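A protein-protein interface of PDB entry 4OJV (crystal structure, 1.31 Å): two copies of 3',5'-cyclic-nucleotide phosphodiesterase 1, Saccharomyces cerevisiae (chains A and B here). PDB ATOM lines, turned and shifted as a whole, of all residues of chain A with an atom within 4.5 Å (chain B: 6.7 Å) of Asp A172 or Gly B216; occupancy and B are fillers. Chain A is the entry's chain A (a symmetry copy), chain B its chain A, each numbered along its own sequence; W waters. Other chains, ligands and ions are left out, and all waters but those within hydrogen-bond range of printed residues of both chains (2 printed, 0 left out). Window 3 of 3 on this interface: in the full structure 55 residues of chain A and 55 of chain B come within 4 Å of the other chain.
The backbone NH of Val B217 lies within hydrogen-bond range of the side-chain carboxylate of Asp A172. The backbone NH (N) of Lys B218 sits at hydrogen-bond distance from the side-chain carboxylate (OD2) of Asp A172 (2.9 Å). The backbone NH (N) of Thr B219 is in hydrogen-bond range of the side-chain carboxylate (OD2) of Asp A172, at 3.2 Å.
The backbone carbonyl oxygen of Gly B214 is in hydrogen-bond range of the backbone NH of Val B223. N of Gly B216 lies within hydrogen-bond range of O of Ala B221 (2.8 Å). The side-chain hydroxyl (OG1) of Thr B219 lies close to the backbone NH (N) of Ala B221 (3.1 Å). OD1 of Asn A171 is in hydrogen-bond range of N of Leu A173 (3.0 Å). The side-chain amide oxygen (OD1) of Asn A171 is in hydrogen-bond range of the backbone NH (N) of Ile A174 (3.0 Å). The side-chain carboxylate (OD1) of Asp A172 sits at hydrogen-bond distance from the backbone NH (N) of Asp A177 (2.8 Å).
Among the printed residues, pairs that only touch across the chains: Asp A172 with Gly B216, Asp A172 with Val B223, Leu A173 with His B130, Ile A174 with His B130, Pro A176 with His B130, Pro A176 with Val B217, Asp A177 with Val B217 and Asp A177 with Lys B218.
Of chain B, only Gly B216 (3.4 Å), Val B217 (2.8 Å), Lys B218 (2.9 Å), Thr B219 (3.2 Å) and Val B223 (3.9 Å) come within 4 Å of Asp A172. Of chain A, only Asp A172 (3.4 Å) comes within 4 Å of Gly B216. Printed residues of chain B within 4 Å of Leu A173: His B130. Of the printed residues of chain B, Ile A174 touches His B130. Of the printed residues of chain A, His B130 touches Leu A173, Ile A174 and Pro A176. Of the printed residues of chain B, Pro A176 touches His B130 (3.9 Å) and Val B217 (3.9 Å). Of the printed residues of chain A, Val B217 touches Asp A172 (2.8 Å), Pro A176 (3.9 Å) and Asp A177 (3.4 Å). Ile B215 touches none of the printed residues of chain A. The nearest residue of chain B that does not touch Asp A172 is His B130 (4.9 Å). The nearest printed residue of chain A that does not touch Gly B216 is Asp A177 (6.0 Å).
Of the 11 printed residues of chain B, 6 touch a printed residue of chain A. Along chain B the printed residues that touch a printed residue of chain A span positions 130 to 223. Among the printed residues, 11 pairs touch across the chains. Among the printed residues, no Asp or Glu carboxylate lies within 4 Å of a Lys or Arg side-chain nitrogen of the other chain.
No position is printed for both chains. Of the 11 pairs that touch across the chains among the printed residues, none has its exchanged pair printed and touching as well.
Water W2 bridges a ring nitrogen (NE2) of His B130 (2.8 Å) and the backbone carbonyl oxygen (O) of Asp A172 (2.9 Å). Water W1 lies within hydrogen-bond range of the backbone carbonyl oxygen (O) of Leu A173 and a ring nitrogen (NE2) of His B130.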
ATOM      1  N   PHE A 170       7.327 -30.242  20.383  1.00  0.00           N
ATOM      2  CA  PHE A 170       6.679 -29.093  19.759  1.00  0.00           C
ATOM      3  C   PHE A 170       5.248 -29.467  19.416  1.00  0.00           C
ATOM      4  O   PHE A 170       4.885 -29.625  18.246  1.00  0.00           O
ATOM      5  CB  PHE A 170       7.472 -28.626  18.540  1.00  0.00           C
ATOM      6  CG  PHE A 170       8.855 -28.168  18.886  1.00  0.00           C
ATOM      7  CD1 PHE A 170       9.057 -26.961  19.543  1.00  0.00           C
ATOM      8  CD2 PHE A 170       9.958 -28.956  18.583  1.00  0.00           C
ATOM      9  CE1 PHE A 170      10.338 -26.544  19.890  1.00  0.00           C
ATOM     10  CE2 PHE A 170      11.236 -28.549  18.924  1.00  0.00           C
ATOM     11  CZ  PHE A 170      11.429 -27.340  19.566  1.00  0.00           C
ATOM     12  N   ASN A 171       4.443 -29.631  20.464  1.00  0.00           N
ATOM     13  CA  ASN A 171       3.130 -30.263  20.333  1.00  0.00           C
ATOM     14  C   ASN A 171       2.030 -29.539  21.102  1.00  0.00           C
ATOM     15  O   ASN A 171       0.961 -30.099  21.328  1.00  0.00           O
ATOM     16  CB  ASN A 171       3.199 -31.742  20.754  1.00  0.00           C
ATOM     17  CG  ASN A 171       3.533 -31.922  22.230  1.00  0.00           C
ATOM     18  OD1 ASN A 171       3.620 -30.951  22.978  1.00  0.00           O
ATOM     19  ND2 ASN A 171       3.686 -33.166  22.658  1.00  0.00           N
ATOM     20  N   ASP A 172       2.300 -28.302  21.520  1.00  0.00           N
ATOM     21  CA  ASP A 172       1.348 -27.467  22.255  1.00  0.00           C
ATOM     22  C   ASP A 172       1.007 -27.969  23.660  1.00  0.00           C
ATOM     23  O   ASP A 172       0.133 -27.415  24.328  1.00  0.00           O
ATOM     24  CB  ASP A 172       0.092 -27.195  21.411  1.00  0.00           C
ATOM     25  CG  ASP A 172       0.390 -26.300  20.234  1.00  0.00           C
ATOM     26  OD1 ASP A 172       1.131 -25.313  20.425  1.00  0.00           O
ATOM     27  OD2 ASP A 172      -0.147 -26.535  19.129  1.00  0.00           O
ATOM     28  N   LEU A 173       1.757 -28.965  24.126  1.00  0.00           N
ATOM     29  CA  LEU A 173       1.576 -29.536  25.456  1.00  0.00           C
ATOM     30  C   LEU A 173       2.873 -29.399  26.275  1.00  0.00           C
ATOM     31  O   LEU A 173       2.898 -28.754  27.321  1.00  0.00           O
ATOM     32  CB  LEU A 173       1.122 -30.998  25.345  1.00  0.00           C
ATOM     33  CG  LEU A 173      -0.180 -31.244  24.572  1.00  0.00           C
ATOM     34  CD1 LEU A 173      -0.324 -32.708  24.189  1.00  0.00           C
ATOM     35  CD2 LEU A 173      -1.403 -30.767  25.351  1.00  0.00           C
ATOM     36  N   ILE A 174       3.956 -29.974  25.757  1.00  0.00           N
ATOM     37  CA  ILE A 174       5.287 -29.827  26.352  1.00  0.00           C
ATOM     38  C   ILE A 174       5.890 -28.462  25.995  1.00  0.00           C
ATOM     39  O   ILE A 174       6.624 -27.859  26.784  1.00  0.00           O
ATOM     40  CB  ILE A 174       6.192 -30.999  25.906  1.00  0.00           C
ATOM     41  CG1 ILE A 174       5.684 -32.323  26.506  1.00  0.00           C
ATOM     42  CG2 ILE A 174       7.661 -30.732  26.244  1.00  0.00           C
ATOM     43  CD1 ILE A 174       5.672 -32.365  28.016  1.00  0.00           C
ATOM     44  N   TRP A 175       5.565 -27.971  24.804  1.00  0.00           N
ATOM     45  CA  TRP A 175       6.020 -26.656  24.357  1.00  0.00           C
ATOM     46  C   TRP A 175       5.096 -26.165  23.280  1.00  0.00           C
ATOM     47  O   TRP A 175       4.587 -26.982  22.507  1.00  0.00           O
ATOM     48  CB  TRP A 175       7.443 -26.742  23.804  1.00  0.00           C
ATOM     49  CG  TRP A 175       8.157 -25.422  23.836  1.00  0.00           C
ATOM     50  CD1 TRP A 175       8.584 -24.653  22.764  1.00  0.00           C
ATOM     51  CD2 TRP A 175       8.551 -24.696  25.036  1.00  0.00           C
ATOM     52  NE1 TRP A 175       9.202 -23.503  23.214  1.00  0.00           N
ATOM     53  CE2 TRP A 175       9.215 -23.479  24.582  1.00  0.00           C
ATOM     54  CE3 TRP A 175       8.415 -24.929  26.398  1.00  0.00           C
ATOM     55  CZ2 TRP A 175       9.737 -22.554  25.474  1.00  0.00           C
ATOM     56  CZ3 TRP A 175       8.925 -23.986  27.288  1.00  0.00           C
ATOM     57  CH2 TRP A 175       9.578 -22.832  26.835  1.00  0.00           C
ATOM     58  N   PRO A 176       4.883 -24.833  23.187  1.00  0.00           N
ATOM     59  CA  PRO A 176       4.124 -24.340  22.034  1.00  0.00           C
ATOM     60  C   PRO A 176       4.731 -24.857  20.737  1.00  0.00           C
ATOM     61  O   PRO A 176       5.964 -24.956  20.613  1.00  0.00           O
ATOM     62  CB  PRO A 176       4.281 -22.823  22.150  1.00  0.00           C
ATOM     63  CG  PRO A 176       4.370 -22.601  23.631  1.00  0.00           C
ATOM     64  CD  PRO A 176       5.244 -23.734  24.105  1.00  0.00           C
ATOM     65  N   ASP A 177       3.871 -25.212  19.781  1.00  0.00           N
ATOM     66  CA  ASP A 177       4.351 -25.781  18.535  1.00  0.00           C
ATOM     67  C   ASP A 177       4.839 -24.669  17.603  1.00  0.00           C
ATOM     68  O   ASP A 177       4.147 -24.240  16.672  1.00  0.00           O
ATOM     69  CB  ASP A 177       3.288 -26.654  17.864  1.00  0.00           C
ATOM     70  CG  ASP A 177       3.816 -27.356  16.628  1.00  0.00           C
ATOM     71  OD1 ASP A 177       4.976 -27.084  16.223  1.00  0.00           O
ATOM     72  OD2 ASP A 177       3.057 -28.179  16.066  1.00  0.00           O
ATOM     73  N   HIS B 130       4.711 -27.638  30.585  1.00  0.00           N
ATOM     74  CA  HIS B 130       5.708 -26.936  29.755  1.00  0.00           C
ATOM     75  C   HIS B 130       7.093 -27.241  30.263  1.00  0.00           C
ATOM     76  O   HIS B 130       7.328 -27.332  31.481  1.00  0.00           O
ATOM     77  CB  HIS B 130       5.516 -25.424  29.745  1.00  0.00           C
ATOM     78  CG  HIS B 130       4.467 -24.931  28.783  1.00  0.00           C
ATOM     79  ND1 HIS B 130       3.878 -23.703  28.916  1.00  0.00           N
ATOM     80  CD2 HIS B 130       3.940 -25.512  27.644  1.00  0.00           C
ATOM     81  CE1 HIS B 130       3.011 -23.538  27.894  1.00  0.00           C
ATOM     82  NE2 HIS B 130       3.038 -24.652  27.132  1.00  0.00           N
ATOM     83  N   GLY B 214      -3.233 -19.682  27.927  1.00  0.00           N
ATOM     84  CA  GLY B 214      -3.106 -19.497  26.485  1.00  0.00           C
ATOM     85  C   GLY B 214      -3.725 -20.625  25.693  1.00  0.00           C
ATOM     86  O   GLY B 214      -4.555 -21.386  26.200  1.00  0.00           O
ATOM     87  N   ILE B 215      -3.311 -20.731  24.439  1.00  0.00           N
ATOM     88  CA  ILE B 215      -3.881 -21.713  23.515  1.00  0.00           C
ATOM     89  C   ILE B 215      -2.778 -22.312  22.654  1.00  0.00           C
ATOM     90  O   ILE B 215      -1.723 -21.697  22.467  1.00  0.00           O
ATOM     91  CB  ILE B 215      -4.991 -21.119  22.606  1.00  0.00           C
ATOM     92  CG1 ILE B 215      -4.435 -19.976  21.748  1.00  0.00           C
ATOM     93  CG2 ILE B 215      -6.195 -20.665  23.426  1.00  0.00           C
ATOM     94  CD1 ILE B 215      -5.376 -19.460  20.679  1.00  0.00           C
ATOM     95  N   GLY B 216      -3.024 -23.507  22.131  1.00  0.00           N
ATOM     96  CA  GLY B 216      -2.070 -24.142  21.234  1.00  0.00           C
ATOM     97  C   GLY B 216      -1.816 -23.318  19.984  1.00  0.00           C
ATOM     98  O   GLY B 216      -2.755 -22.777  19.395  1.00  0.00           O
ATOM     99  N   VAL B 217      -0.554 -23.244  19.559  1.00  0.00           N
ATOM    100  CA  VAL B 217      -0.191 -22.581  18.310  1.00  0.00           C
ATOM    101  C   VAL B 217      -0.796 -23.307  17.111  1.00  0.00           C
ATOM    102  O   VAL B 217      -1.395 -22.670  16.237  1.00  0.00           O
ATOM    103  CB  VAL B 217       1.344 -22.495  18.160  1.00  0.00           C
ATOM    104  CG1 VAL B 217       1.725 -21.907  16.807  1.00  0.00           C
ATOM    105  CG2 VAL B 217       1.957 -21.680  19.297  1.00  0.00           C
ATOM    106  N   LYS B 218      -0.644 -24.628  17.065  1.00  0.00           N
ATOM    107  CA  LYS B 218      -1.214 -25.426  15.977  1.00  0.00           C
ATOM    108  C   LYS B 218      -2.661 -25.783  16.283  1.00  0.00           C
ATOM    109  O   LYS B 218      -3.532 -25.665  15.424  1.00  0.00           O
ATOM    110  CB  LYS B 218      -0.398 -26.707  15.739  1.00  0.00           C
ATOM    111  CG  LYS B 218      -0.742 -27.441  14.447  1.00  0.00           C
ATOM    112  CD  LYS B 218      -0.008 -28.770  14.346  1.00  0.00           C
ATOM    113  CE  LYS B 218       0.027 -29.298  12.918  1.00  0.00           C
ATOM    114  NZ  LYS B 218      -1.333 -29.627  12.413  1.00  0.00           N
ATOM    115  N   THR B 219      -2.922 -26.234  17.503  1.00  0.00           N
ATOM    116  CA  THR B 219      -4.202 -26.875  17.794  1.00  0.00           C
ATOM    117  C   THR B 219      -5.289 -25.896  18.180  1.00  0.00           C
ATOM    118  O   THR B 219      -6.468 -26.247  18.120  1.00  0.00           O
ATOM    119  CB  THR B 219      -4.078 -27.872  18.942  1.00  0.00           C
ATOM    120  OG1 THR B 219      -3.706 -27.142  20.116  1.00  0.00           O
ATOM    121  CG2 THR B 219      -3.049 -28.951  18.613  1.00  0.00           C
ATOM    122  N   GLY B 220      -4.914 -24.690  18.601  1.00  0.00           N
ATOM    123  CA  GLY B 220      -5.867 -23.743  19.157  1.00  0.00           C
ATOM    124  C   GLY B 220      -6.540 -24.193  20.445  1.00  0.00           C
ATOM    125  O   GLY B 220      -7.455 -23.523  20.925  1.00  0.00           O
ATOM    126  N   ALA B 221      -6.099 -25.318  21.010  1.00  0.00           N
ATOM    127  CA  ALA B 221      -6.739 -25.885  22.199  1.00  0.00           C
ATOM    128  C   ALA B 221      -6.360 -25.078  23.443  1.00  0.00           C
ATOM    129  O   ALA B 221      -5.247 -24.556  23.523  1.00  0.00           O
ATOM    130  CB  ALA B 221      -6.354 -27.345  22.364  1.00  0.00           C
ATOM    131  N   PRO B 222      -7.274 -24.966  24.427  1.00  0.00           N
ATOM    132  CA  PRO B 222      -6.898 -24.277  25.667  1.00  0.00           C
ATOM    133  C   PRO B 222      -5.705 -24.971  26.315  1.00  0.00           C
ATOM    134  O   PRO B 222      -5.669 -26.195  26.383  1.00  0.00           O
ATOM    135  CB  PRO B 222      -8.147 -24.418  26.552  1.00  0.00           C
ATOM    136  CG  PRO B 222      -9.263 -24.753  25.623  1.00  0.00           C
ATOM    137  CD  PRO B 222      -8.649 -25.499  24.473  1.00  0.00           C
ATOM    138  N   VAL B 223      -4.729 -24.179  26.760  1.00  0.00           N
ATOM    139  CA  VAL B 223      -3.567 -24.666  27.503  1.00  0.00           C
ATOM    140  C   VAL B 223      -3.826 -24.312  28.954  1.00  0.00           C
ATOM    141  O   VAL B 223      -3.923 -23.141  29.295  1.00  0.00           O
ATOM    142  CB  VAL B 223      -2.262 -23.997  27.005  1.00  0.00           C
ATOM    143  CG1 VAL B 223      -1.078 -24.351  27.903  1.00  0.00           C
ATOM    144  CG2 VAL B 223      -1.990 -24.392  25.555  1.00  0.00           C
HETATM  145  O   HOH W   1       1.520 -26.926  29.117  1.00  0.00           O
HETATM  146  O   HOH W   2       1.601 -24.939  24.711  1.00  0.00           O
